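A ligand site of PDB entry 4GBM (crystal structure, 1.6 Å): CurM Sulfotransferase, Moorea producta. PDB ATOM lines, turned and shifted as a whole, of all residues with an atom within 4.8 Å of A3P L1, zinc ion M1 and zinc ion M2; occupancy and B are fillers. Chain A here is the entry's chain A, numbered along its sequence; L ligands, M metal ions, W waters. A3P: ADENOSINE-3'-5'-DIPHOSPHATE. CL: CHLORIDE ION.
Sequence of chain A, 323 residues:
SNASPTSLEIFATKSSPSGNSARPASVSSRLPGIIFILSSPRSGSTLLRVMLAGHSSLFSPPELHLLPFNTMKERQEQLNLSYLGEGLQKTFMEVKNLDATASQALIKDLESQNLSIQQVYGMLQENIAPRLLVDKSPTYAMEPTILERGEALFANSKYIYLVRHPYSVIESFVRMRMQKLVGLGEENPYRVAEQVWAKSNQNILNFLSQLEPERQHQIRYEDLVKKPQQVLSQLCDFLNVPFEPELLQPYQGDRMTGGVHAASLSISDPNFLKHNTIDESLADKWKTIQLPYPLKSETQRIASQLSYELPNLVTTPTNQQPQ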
ATOM      1  N   SER A  40     -23.400 -11.233 -28.817  1.00  0.00           N
ATOM      2  CA  SER A  40     -22.100 -10.789 -29.314  1.00  0.00           C
ATOM      3  C   SER A  40     -21.047 -11.825 -28.891  1.00  0.00           C
ATOM      4  O   SER A  40     -21.239 -12.534 -27.900  1.00  0.00           O
ATOM      5  CB  SER A  40     -21.760  -9.424 -28.700  1.00  0.00           C
ATOM      6  OG  SER A  40     -20.389  -9.089 -28.826  1.00  0.00           O
ATOM      7  N   PRO A  41     -19.928 -11.917 -29.640  1.00  0.00           N
ATOM      8  CA  PRO A  41     -18.786 -12.695 -29.132  1.00  0.00           C
ATOM      9  C   PRO A  41     -18.392 -12.299 -27.704  1.00  0.00           C
ATOM     10  O   PRO A  41     -18.631 -11.159 -27.292  1.00  0.00           O
ATOM     11  CB  PRO A  41     -17.674 -12.280 -30.101  1.00  0.00           C
ATOM     12  CG  PRO A  41     -18.391 -12.107 -31.387  1.00  0.00           C
ATOM     13  CD  PRO A  41     -19.668 -11.398 -30.995  1.00  0.00           C
ATOM     14  N   ARG A  42     -17.799 -13.236 -26.969  1.00  0.00           N
ATOM     15  CA  ARG A  42     -17.193 -13.005 -25.650  1.00  0.00           C
ATOM     16  C   ARG A  42     -18.195 -12.646 -24.543  1.00  0.00           C
ATOM     17  O   ARG A  42     -17.832 -11.983 -23.564  1.00  0.00           O
ATOM     18  CB  ARG A  42     -16.051 -11.939 -25.704  1.00  0.00           C
ATOM     19  CG  ARG A  42     -15.137 -12.021 -26.933  1.00  0.00           C
ATOM     20  CD  ARG A  42     -14.600 -13.425 -27.143  1.00  0.00           C
ATOM     21  NE  ARG A  42     -13.809 -13.916 -26.009  1.00  0.00           N
ATOM     22  CZ  ARG A  42     -13.267 -15.128 -25.974  1.00  0.00           C
ATOM     23  NH1 ARG A  42     -12.546 -15.510 -24.921  1.00  0.00           N
ATOM     24  NH2 ARG A  42     -13.456 -15.962 -26.991  1.00  0.00           N
ATOM     25  N   SER A  43     -19.442 -13.096 -24.684  1.00  0.00           N
ATOM     26  CA  SER A  43     -20.509 -12.713 -23.758  1.00  0.00           C
ATOM     27  C   SER A  43     -20.885 -13.815 -22.766  1.00  0.00           C
ATOM     28  O   SER A  43     -21.888 -13.693 -22.074  1.00  0.00           O
ATOM     29  CB  SER A  43     -21.755 -12.264 -24.532  1.00  0.00           C
ATOM     30  OG  SER A  43     -21.459 -11.117 -25.313  1.00  0.00           O
ATOM     31  N   GLY A  44     -20.057 -14.859 -22.706  1.00  0.00           N
ATOM     32  CA  GLY A  44     -20.332 -16.018 -21.842  1.00  0.00           C
ATOM     33  C   GLY A  44     -21.302 -17.001 -22.488  1.00  0.00           C
ATOM     34  O   GLY A  44     -21.978 -17.776 -21.782  1.00  0.00           O
ATOM     35  N   SER A  45     -21.393 -16.986 -23.814  1.00  0.00           N
ATOM     36  CA  SER A  45     -22.346 -17.855 -24.531  1.00  0.00           C
ATOM     37  C   SER A  45     -22.019 -19.340 -24.354  1.00  0.00           C
ATOM     38  O   SER A  45     -22.932 -20.161 -24.199  1.00  0.00           O
ATOM     39  CB  SER A  45     -22.454 -17.487 -26.019  1.00  0.00           C
ATOM     40  OG  SER A  45     -21.260 -17.790 -26.724  1.00  0.00           O
ATOM     41  N   THR A  46     -20.734 -19.692 -24.346  1.00  0.00           N
ATOM     42  CA  THR A  46     -20.308 -21.084 -24.160  1.00  0.00           C
ATOM     43  C   THR A  46     -20.667 -21.554 -22.754  1.00  0.00           C
ATOM     44  O   THR A  46     -21.238 -22.632 -22.577  1.00  0.00           O
ATOM     45  CB  THR A  46     -18.815 -21.277 -24.467  1.00  0.00           C
ATOM     46  OG1 THR A  46     -18.552 -20.830 -25.794  1.00  0.00           O
ATOM     47  CG2 THR A  46     -18.423 -22.762 -24.337  1.00  0.00           C
ATOM     48  N   LEU A  47     -20.347 -20.738 -21.756  1.00  0.00           N
ATOM     49  CA  LEU A  47     -20.765 -21.051 -20.383  1.00  0.00           C
ATOM     50  C   LEU A  47     -22.264 -21.358 -20.319  1.00  0.00           C
ATOM     51  O   LEU A  47     -22.665 -22.385 -19.782  1.00  0.00           O
ATOM     52  CB  LEU A  47     -20.407 -19.911 -19.437  1.00  0.00           C
ATOM     53  CG  LEU A  47     -20.941 -20.053 -18.009  1.00  0.00           C
ATOM     54  CD1 LEU A  47     -20.278 -21.219 -17.264  1.00  0.00           C
ATOM     55  CD2 LEU A  47     -20.714 -18.742 -17.268  1.00  0.00           C
ATOM     56  N   LYS A 136     -26.625 -22.405 -30.302  1.00  0.00           N
ATOM     57  CA  LYS A 136     -25.861 -21.213 -29.922  1.00  0.00           C
ATOM     58  C   LYS A 136     -24.715 -20.932 -30.885  1.00  0.00           C
ATOM     59  O   LYS A 136     -23.904 -21.818 -31.174  1.00  0.00           O
ATOM     60  CB  LYS A 136     -25.274 -21.383 -28.506  1.00  0.00           C
ATOM     61  CG  LYS A 136     -24.541 -20.134 -27.937  1.00  0.00           C
ATOM     62  CD  LYS A 136     -23.046 -20.030 -28.374  1.00  0.00           C
ATOM     63  CE  LYS A 136     -22.134 -20.948 -27.555  1.00  0.00           C
ATOM     64  NZ  LYS A 136     -20.707 -20.581 -27.814  1.00  0.00           N
ATOM     65  N   PRO A 138     -22.294 -17.047 -31.580  1.00  0.00           N
ATOM     66  CA  PRO A 138     -22.236 -15.582 -31.634  1.00  0.00           C
ATOM     67  C   PRO A 138     -22.225 -15.044 -33.062  1.00  0.00           C
ATOM     68  O   PRO A 138     -22.567 -13.867 -33.282  1.00  0.00           O
ATOM     69  CB  PRO A 138     -20.921 -15.258 -30.924  1.00  0.00           C
ATOM     70  CG  PRO A 138     -20.657 -16.398 -30.052  1.00  0.00           C
ATOM     71  CD  PRO A 138     -21.162 -17.606 -30.819  1.00  0.00           C
ATOM     72  N   ARG A 164     -23.588  -8.718 -22.611  1.00  0.00           N
ATOM     73  CA  ARG A 164     -22.507  -8.420 -21.656  1.00  0.00           C
ATOM     74  C   ARG A 164     -22.052  -6.978 -21.859  1.00  0.00           C
ATOM     75  O   ARG A 164     -22.170  -6.442 -22.954  1.00  0.00           O
ATOM     76  CB  ARG A 164     -21.350  -9.406 -21.843  1.00  0.00           C
ATOM     77  CG  ARG A 164     -20.266  -9.259 -20.773  1.00  0.00           C
ATOM     78  CD  ARG A 164     -19.207 -10.313 -20.930  1.00  0.00           C
ATOM     79  NE  ARG A 164     -18.262 -10.242 -19.809  1.00  0.00           N
ATOM     80  CZ  ARG A 164     -17.149 -10.960 -19.739  1.00  0.00           C
ATOM     81  NH1 ARG A 164     -16.819 -11.777 -20.742  1.00  0.00           N
ATOM     82  NH2 ARG A 164     -16.361 -10.869 -18.673  1.00  0.00           N
ATOM     83  N   SER A 172     -11.925  -8.370 -23.962  1.00  0.00           N
ATOM     84  CA  SER A 172     -11.747  -9.780 -24.247  1.00  0.00           C
ATOM     85  C   SER A 172     -11.440 -10.018 -25.736  1.00  0.00           C
ATOM     86  O   SER A 172     -10.497 -10.725 -26.073  1.00  0.00           O
ATOM     87  CB  SER A 172     -13.005 -10.562 -23.842  1.00  0.00           C
ATOM     88  OG  SER A 172     -12.888 -11.924 -24.210  1.00  0.00           O
ATOM     89  N   ARG A 175      -7.898  -8.865 -26.459  1.00  0.00           N
ATOM     90  CA  ARG A 175      -6.958  -9.786 -25.797  1.00  0.00           C
ATOM     91  C   ARG A 175      -6.807 -11.097 -26.570  1.00  0.00           C
ATOM     92  O   ARG A 175      -5.695 -11.650 -26.669  1.00  0.00           O
ATOM     93  CB  ARG A 175      -7.410 -10.046 -24.357  1.00  0.00           C
ATOM     94  CG  ARG A 175      -6.598 -11.128 -23.613  1.00  0.00           C
ATOM     95  CD  ARG A 175      -6.786 -11.103 -22.084  1.00  0.00           C
ATOM     96  NE  ARG A 175      -8.159 -10.805 -21.683  1.00  0.00           N
ATOM     97  CZ  ARG A 175      -9.179 -11.659 -21.765  1.00  0.00           C
ATOM     98  NH1 ARG A 175     -10.398 -11.270 -21.387  1.00  0.00           N
ATOM     99  NH2 ARG A 175      -8.996 -12.894 -22.226  1.00  0.00           N
ATOM    100  N   MET A 176      -7.921 -11.583 -27.116  1.00  0.00           N
ATOM    101  CA  MET A 176      -7.955 -12.856 -27.840  1.00  0.00           C
ATOM    102  C   MET A 176      -7.534 -12.715 -29.302  1.00  0.00           C
ATOM    103  O   MET A 176      -7.464 -13.704 -30.039  1.00  0.00           O
ATOM    104  CB  MET A 176      -9.337 -13.506 -27.726  1.00  0.00           C
ATOM    105  CG  MET A 176      -9.724 -13.894 -26.287  1.00  0.00           C
ATOM    106  SD  MET A 176      -8.547 -15.011 -25.519  1.00  0.00           S
ATOM    107  CE  MET A 176      -8.780 -16.493 -26.515  1.00  0.00           C
ATOM    108  N   TYR A 221     -25.062 -11.301 -18.803  1.00  0.00           N
ATOM    109  CA  TYR A 221     -23.917 -12.092 -18.365  1.00  0.00           C
ATOM    110  C   TYR A 221     -23.587 -11.833 -16.899  1.00  0.00           C
ATOM    111  O   TYR A 221     -23.267 -12.759 -16.137  1.00  0.00           O
ATOM    112  CB  TYR A 221     -22.685 -11.794 -19.226  1.00  0.00           C
ATOM    113  CG  TYR A 221     -21.428 -12.395 -18.653  1.00  0.00           C
ATOM    114  CD1 TYR A 221     -21.113 -13.737 -18.871  1.00  0.00           C
ATOM    115  CD2 TYR A 221     -20.565 -11.631 -17.870  1.00  0.00           C
ATOM    116  CE1 TYR A 221     -19.968 -14.296 -18.333  1.00  0.00           C
ATOM    117  CE2 TYR A 221     -19.406 -12.174 -17.327  1.00  0.00           C
ATOM    118  CZ  TYR A 221     -19.105 -13.511 -17.561  1.00  0.00           C
ATOM    119  OH  TYR A 221     -17.965 -14.039 -17.015  1.00  0.00           O
ATOM    120  N   VAL A 225     -23.512 -14.859 -13.939  1.00  0.00           N
ATOM    121  CA  VAL A 225     -22.401 -15.370 -13.131  1.00  0.00           C
ATOM    122  C   VAL A 225     -22.466 -14.970 -11.653  1.00  0.00           C
ATOM    123  O   VAL A 225     -21.898 -15.667 -10.793  1.00  0.00           O
ATOM    124  CB  VAL A 225     -21.010 -15.078 -13.759  1.00  0.00           C
ATOM    125  CG1 VAL A 225     -20.940 -15.639 -15.177  1.00  0.00           C
ATOM    126  CG2 VAL A 225     -20.702 -13.568 -13.751  1.00  0.00           C
ATOM    127  N   TYR A 251     -19.296 -28.035 -14.941  1.00  0.00           N
ATOM    128  CA  TYR A 251     -18.049 -28.828 -14.973  1.00  0.00           C
ATOM    129  C   TYR A 251     -18.247 -30.301 -14.622  1.00  0.00           C
ATOM    130  O   TYR A 251     -17.274 -31.040 -14.433  1.00  0.00           O
ATOM    131  CB  TYR A 251     -16.967 -28.160 -14.103  1.00  0.00           C
ATOM    132  CG  TYR A 251     -16.534 -26.843 -14.686  1.00  0.00           C
ATOM    133  CD1 TYR A 251     -15.534 -26.785 -15.657  1.00  0.00           C
ATOM    134  CD2 TYR A 251     -17.168 -25.656 -14.317  1.00  0.00           C
ATOM    135  CE1 TYR A 251     -15.153 -25.566 -16.232  1.00  0.00           C
ATOM    136  CE2 TYR A 251     -16.805 -24.443 -14.877  1.00  0.00           C
ATOM    137  CZ  TYR A 251     -15.793 -24.407 -15.829  1.00  0.00           C
ATOM    138  OH  TYR A 251     -15.439 -23.199 -16.388  1.00  0.00           O
ATOM    139  N   PRO A 270     -13.230 -19.930 -25.869  1.00  0.00           N
ATOM    140  CA  PRO A 270     -14.093 -19.297 -24.865  1.00  0.00           C
ATOM    141  C   PRO A 270     -13.483 -19.313 -23.463  1.00  0.00           C
ATOM    142  O   PRO A 270     -14.014 -18.683 -22.550  1.00  0.00           O
ATOM    143  CB  PRO A 270     -15.363 -20.140 -24.904  1.00  0.00           C
ATOM    144  CG  PRO A 270     -14.946 -21.466 -25.401  1.00  0.00           C
ATOM    145  CD  PRO A 270     -13.786 -21.210 -26.359  1.00  0.00           C
ATOM    146  N   ASN A 271     -12.370 -20.044 -23.304  1.00  0.00           N
ATOM    147  CA  ASN A 271     -11.619 -20.109 -22.051  1.00  0.00           C
ATOM    148  C   ASN A 271     -12.393 -20.760 -20.913  1.00  0.00           C
ATOM    149  O   ASN A 271     -12.057 -20.585 -19.740  1.00  0.00           O
ATOM    150  CB  ASN A 271     -11.083 -18.727 -21.640  1.00  0.00           C
ATOM    151  CG  ASN A 271     -10.103 -18.164 -22.658  1.00  0.00           C
ATOM    152  OD1 ASN A 271      -9.294 -18.895 -23.242  1.00  0.00           O
ATOM    153  ND2 ASN A 271     -10.181 -16.845 -22.885  1.00  0.00           N
ATOM    154  N   PHE A 272     -13.410 -21.514 -21.287  1.00  0.00           N
ATOM    155  CA  PHE A 272     -14.253 -22.223 -20.328  1.00  0.00           C
ATOM    156  C   PHE A 272     -13.418 -23.161 -19.459  1.00  0.00           C
ATOM    157  O   PHE A 272     -13.604 -23.236 -18.244  1.00  0.00           O
ATOM    158  CB  PHE A 272     -15.380 -22.968 -21.071  1.00  0.00           C
ATOM    159  CG  PHE A 272     -16.212 -23.841 -20.188  1.00  0.00           C
ATOM    160  CD1 PHE A 272     -17.173 -23.274 -19.335  1.00  0.00           C
ATOM    161  CD2 PHE A 272     -16.046 -25.222 -20.197  1.00  0.00           C
ATOM    162  CE1 PHE A 272     -17.938 -24.082 -18.497  1.00  0.00           C
ATOM    163  CE2 PHE A 272     -16.808 -26.038 -19.365  1.00  0.00           C
ATOM    164  CZ  PHE A 272     -17.760 -25.467 -18.512  1.00  0.00           C
ATOM    165  N   LYS A 274     -10.392 -22.841 -18.586  1.00  0.00           N
ATOM    166  CA  LYS A 274      -9.459 -22.120 -17.719  1.00  0.00           C
ATOM    167  C   LYS A 274     -10.102 -21.761 -16.371  1.00  0.00           C
ATOM    168  O   LYS A 274      -9.456 -21.140 -15.513  1.00  0.00           O
ATOM    169  CB  LYS A 274      -8.892 -20.881 -18.418  1.00  0.00           C
ATOM    170  CG  LYS A 274      -7.929 -21.231 -19.543  1.00  0.00           C
ATOM    171  CD  LYS A 274      -7.388 -19.984 -20.216  1.00  0.00           C
ATOM    172  CE  LYS A 274      -6.530 -20.333 -21.426  1.00  0.00           C
ATOM    173  NZ  LYS A 274      -7.352 -20.875 -22.552  1.00  0.00           N
ATOM    174  N   HIS A 275     -11.350 -22.182 -16.193  1.00  0.00           N
ATOM    175  CA  HIS A 275     -12.067 -22.018 -14.934  1.00  0.00           C
ATOM    176  C   HIS A 275     -12.537 -23.380 -14.437  1.00  0.00           C
ATOM    177  O   HIS A 275     -12.477 -24.374 -15.174  1.00  0.00           O
ATOM    178  CB  HIS A 275     -13.247 -21.044 -15.120  1.00  0.00           C
ATOM    179  CG  HIS A 275     -12.820 -19.712 -15.656  1.00  0.00           C
ATOM    180  ND1 HIS A 275     -12.386 -18.692 -14.842  1.00  0.00           N
ATOM    181  CD2 HIS A 275     -12.747 -19.238 -16.925  1.00  0.00           C
ATOM    182  CE1 HIS A 275     -12.066 -17.635 -15.576  1.00  0.00           C
ATOM    183  NE2 HIS A 275     -12.266 -17.955 -16.844  1.00  0.00           N
ATOM    184  N   THR A 277     -15.417 -23.306 -11.999  1.00  0.00           N
ATOM    185  CA  THR A 277     -16.714 -22.986 -11.417  1.00  0.00           C
ATOM    186  C   THR A 277     -17.341 -21.854 -12.219  1.00  0.00           C
ATOM    187  O   THR A 277     -16.690 -21.292 -13.102  1.00  0.00           O
ATOM    188  CB  THR A 277     -16.583 -22.594  -9.915  1.00  0.00           C
ATOM    189  OG1 THR A 277     -17.888 -22.526  -9.322  1.00  0.00           O
ATOM    190  CG2 THR A 277     -15.857 -21.258  -9.752  1.00  0.00           C
ATOM    191  N   ILE A 278     -18.591 -21.521 -11.912  1.00  0.00           N
ATOM    192  CA  ILE A 278     -19.204 -20.304 -12.463  1.00  0.00           C
ATOM    193  C   ILE A 278     -18.505 -19.131 -11.759  1.00  0.00           C
ATOM    194  O   ILE A 278     -18.715 -18.914 -10.557  1.00  0.00           O
ATOM    195  CB  ILE A 278     -20.714 -20.261 -12.214  1.00  0.00           C
ATOM    196  CG1 ILE A 278     -21.384 -21.485 -12.849  1.00  0.00           C
ATOM    197  CG2 ILE A 278     -21.315 -18.957 -12.767  1.00  0.00           C
ATOM    198  CD1 ILE A 278     -22.815 -21.756 -12.364  1.00  0.00           C
ATOM    199  N   ASP A 279     -17.666 -18.417 -12.496  1.00  0.00           N
ATOM    200  CA  ASP A 279     -16.730 -17.478 -11.865  1.00  0.00           C
ATOM    201  C   ASP A 279     -17.313 -16.067 -11.853  1.00  0.00           C
ATOM    202  O   ASP A 279     -17.298 -15.363 -12.859  1.00  0.00           O
ATOM    203  CB  ASP A 279     -15.364 -17.521 -12.560  1.00  0.00           C
ATOM    204  CG  ASP A 279     -14.310 -16.698 -11.844  1.00  0.00           C
ATOM    205  OD1 ASP A 279     -14.687 -15.845 -11.009  1.00  0.00           O
ATOM    206  OD2 ASP A 279     -13.114 -16.919 -12.103  1.00  0.00           O
ATOM    207  N   LEU A 282     -15.681 -12.326 -12.992  1.00  0.00           N
ATOM    208  CA  LEU A 282     -15.569 -11.803 -14.355  1.00  0.00           C
ATOM    209  C   LEU A 282     -16.685 -10.814 -14.699  1.00  0.00           C
ATOM    210  O   LEU A 282     -16.602 -10.091 -15.705  1.00  0.00           O
ATOM    211  CB  LEU A 282     -15.540 -12.959 -15.358  1.00  0.00           C
ATOM    212  CG  LEU A 282     -14.180 -13.641 -15.593  1.00  0.00           C
ATOM    213  CD1 LEU A 282     -13.413 -13.959 -14.312  1.00  0.00           C
ATOM    214  CD2 LEU A 282     -14.350 -14.898 -16.442  1.00  0.00           C
ATOM    215  N   LYS A 285     -15.719  -6.668 -14.226  1.00  0.00           N
ATOM    216  CA  LYS A 285     -14.483  -6.199 -14.867  1.00  0.00           C
ATOM    217  C   LYS A 285     -14.646  -4.842 -15.538  1.00  0.00           C
ATOM    218  O   LYS A 285     -13.713  -4.046 -15.557  1.00  0.00           O
ATOM    219  CB  LYS A 285     -13.955  -7.233 -15.847  1.00  0.00           C
ATOM    220  CG  LYS A 285     -13.350  -8.440 -15.118  1.00  0.00           C
ATOM    221  CD  LYS A 285     -12.998  -9.565 -16.068  1.00  0.00           C
ATOM    222  CE  LYS A 285     -11.697  -9.302 -16.804  1.00  0.00           C
ATOM    223  NZ  LYS A 285     -11.193 -10.565 -17.403  1.00  0.00           N
HETATM  224  P1  A3P L   1     -12.480 -14.300 -21.538  1.00  0.00           P
HETATM  225  O1P A3P L   1     -11.745 -13.755 -22.738  1.00  0.00           O
HETATM  226  O2P A3P L   1     -11.990 -15.662 -21.103  1.00  0.00           O
HETATM  227  O3P A3P L   1     -12.620 -13.293 -20.440  1.00  0.00           O
HETATM  228  P2  A3P L   1     -18.111 -16.730 -25.337  1.00  0.00           P
HETATM  229  O4P A3P L   1     -19.389 -16.045 -25.697  1.00  0.00           O
HETATM  230  O5P A3P L   1     -16.979 -16.553 -26.295  1.00  0.00           O
HETATM  231  O6P A3P L   1     -18.313 -18.162 -24.901  1.00  0.00           O
HETATM  232  O5' A3P L   1     -17.601 -15.948 -24.013  1.00  0.00           O
HETATM  233  C5' A3P L   1     -16.280 -16.193 -23.519  1.00  0.00           C
HETATM  234  C4' A3P L   1     -16.197 -15.520 -22.173  1.00  0.00           C
HETATM  235  O4' A3P L   1     -17.004 -16.258 -21.243  1.00  0.00           O
HETATM  236  C3' A3P L   1     -14.807 -15.580 -21.581  1.00  0.00           C
HETATM  237  O3' A3P L   1     -13.985 -14.522 -22.111  1.00  0.00           O
HETATM  238  C2' A3P L   1     -15.108 -15.444 -20.094  1.00  0.00           C
HETATM  239  O2' A3P L   1     -15.154 -14.065 -19.704  1.00  0.00           O
HETATM  240  C1' A3P L   1     -16.503 -16.042 -19.933  1.00  0.00           C
HETATM  241  N9  A3P L   1     -16.422 -17.344 -19.227  1.00  0.00           N
HETATM  242  C8  A3P L   1     -15.957 -18.518 -19.700  1.00  0.00           C
HETATM  243  N7  A3P L   1     -16.009 -19.488 -18.753  1.00  0.00           N
HETATM  244  C5  A3P L   1     -16.522 -18.920 -17.640  1.00  0.00           C
HETATM  245  C6  A3P L   1     -16.862 -19.365 -16.275  1.00  0.00           C
HETATM  246  N6  A3P L   1     -16.659 -20.652 -15.904  1.00  0.00           N
HETATM  247  N1  A3P L   1     -17.388 -18.437 -15.419  1.00  0.00           N
HETATM  248  C2  A3P L   1     -17.609 -17.159 -15.789  1.00  0.00           C
HETATM  249  N3  A3P L   1     -17.329 -16.692 -17.025  1.00  0.00           N
HETATM  250  C4  A3P L   1     -16.801 -17.521 -17.957  1.00  0.00           C
HETATM  251 CL    CL L   2     -12.671 -20.420 -11.651  1.00  0.00          CL
HETATM  252 CL    CL L   3     -14.862 -18.518 -28.425  1.00  0.00          CL
HETATM  253 CL    CL L   4     -18.456 -18.650 -28.656  1.00  0.00          CL
HETATM  254 CL    CL L   5     -16.570 -15.514 -29.414  1.00  0.00          CL
HETATM  255 ZN    ZN M   1     -12.146 -18.554 -12.752  1.00  0.00          ZN
HETATM  256 ZN    ZN M   2     -16.745 -17.324 -28.133  1.00  0.00          ZN
HETATM  257  O   HOH W   1     -21.096 -14.686 -26.819  1.00  0.00           O
HETATM  258  O   HOH W   2     -11.252 -16.272 -18.787  1.00  0.00           O
HETATM  259  O   HOH W   3     -13.487 -11.154 -19.155  1.00  0.00           O
HETATM  260  O   HOH W   4     -18.283 -18.714 -22.250  1.00  0.00           O
HETATM  261  O   HOH W   5     -10.597 -13.372 -18.480  1.00  0.00           O
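The backbone NH (N) of Asp 279 sits at hydrogen-bond distance from a nitrogen (N1) of A3P L1, 2.9 Å away. The side-chain hydroxyl (OG) of Ser 172 lies within hydrogen-bond range of an oxygen (O1P) of A3P L1. The side-chain hydroxyl (OH) of Tyr 221 lies within hydrogen-bond range of a nitrogen (N3) of A3P L1, 2.7 Å away. N of Ser 45 sits at hydrogen-bond distance from O4P of A3P L1. The side-chain hydroxyl of Ser 45 is in hydrogen-bond range of an oxygen (O4P) of A3P L1. O2P of A3P L1 is in hydrogen-bond range of ND2 of Asn 271. An oxygen (O6P) of A3P L1 sits at hydrogen-bond distance from the backbone NH (N) of Thr 46 (2.9 Å). The side-chain hydroxyl of Thr 46 lies within hydrogen-bond range of an oxygen (O6P) of A3P L1 (2.8 Å). The side-chain hydroxyl of Tyr 251 sits at hydrogen-bond distance from a nitrogen (N6) of A3P L1, at 2.9 Å. N6 of A3P L1 is in hydrogen-bond range of O of Thr 277. An oxygen (O4P) of A3P L1 lies within hydrogen-bond range of the backbone NH (N) of Arg 42, 3.5 Å away. The guanidinium group (NH1) of Arg 42 lies within salt-bridge range of an oxygen (O1P) of A3P L1 (2.9 Å). The guanidinium group of Arg 175 is in salt-bridge range of an oxygen (O1P) of A3P L1 (2.9 Å). O5' of A3P L1 is in hydrogen-bond range of N of Gly 44, at 3.0 Å. An oxygen (O2') of A3P L1 is in hydrogen-bond range of the guanidinium group of Arg 164, 3.0 Å away. An oxygen (O4P) of A3P L1 is in hydrogen-bond range of the backbone NH of Ser 43 (3.1 Å).
OH of Tyr 251 sits close to O of His 275 (3.4 Å). The side-chain hydroxyl of Ser 172 sits at hydrogen-bond distance from the guanidinium group of Arg 42, 2.8 Å away. The side-chain hydroxyl of Ser 45 sits at hydrogen-bond distance from the side-chain amino group of Lys 136 (3.0 Å). The side-chain amide nitrogen of Asn 271 sits at hydrogen-bond distance from the side-chain sulfur of Met 176. The side-chain hydroxyl of Thr 46 sits at hydrogen-bond distance from the side-chain amino group of Lys 136 (3.0 Å). The backbone carbonyl oxygen (O) of Arg 42 lies within hydrogen-bond range of the guanidinium group (NH1) of Arg 164 (3.0 Å). OG of Ser 43 is in hydrogen-bond range of O of Pro 41 (3.5 Å). The side-chain hydroxyl of Ser 43 sits at hydrogen-bond distance from the backbone carbonyl oxygen of Ser 40, at 3.0 Å.
Leu 47 touches A3P L1 (CD2 to C2, 3.8 Å). CG1 of Val 225 touches C2 of A3P L1 (3.7 Å). Pro 270 touches A3P L1 (O to C3', 3.3 Å). Phe 272 touches A3P L1. Ile 278 touches A3P L1. Leu 282 touches A3P L1. Hydrophobic or aromatic side chains that line A3P L1: Leu 47, Tyr 221, Val 225, Tyr 251, Pro 270, His 275 and Leu 282.
NH2 of Arg 42 touches zinc ion M2, 3.7 Å away. Of the 27 residues printed, 1 comes within 4 Å of zinc ion M2. The nearest printed residue that does not touch zinc ion M2 is Pro 138 (4.5 Å).
Zinc ion M1 is bound by OD2 of Asp 279. ND1 of His 275 is bound to zinc ion M1 (2.1 Å). A chlorine (CL) of CL L2 is bound to zinc ion M1 (2.2 Å).
Zinc ion M2 is bound by O5P of A3P L1, CL of CL L5, CL of CL L4 and CL of CL L3. Zinc ion M2 has four donor atoms within binding distance.
Water W1 lies within hydrogen-bond range of O of Ser 40 (2.4 Å), O4P of A3P L1 (2.5 Å), OG of Ser 45 (3.1 Å) and N of Ser 43 (3.1 Å). Water W2 lies within hydrogen-bond range of an oxygen (O2P) of A3P L1 (2.5 Å) and a ring nitrogen (NE2) of His 275 (2.8 Å). Water W3 lies within hydrogen-bond range of an oxygen (O3P) of A3P L1 (2.6 Å), the guanidinium group (NH2) of Arg 164 (2.9 Å) and the side-chain amino group (NZ) of Lys 285 (2.9 Å). Water W4 lies within hydrogen-bond range of O6P of A3P L1 (2.7 Å), N of Leu 47 (2.9 Å) and N of Thr 46 (3.4 Å). Water W5 bridges an oxygen (O3P) of A3P L1 (2.8 Å) and the side-chain amino group of Lys 285 (3.1 Å).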
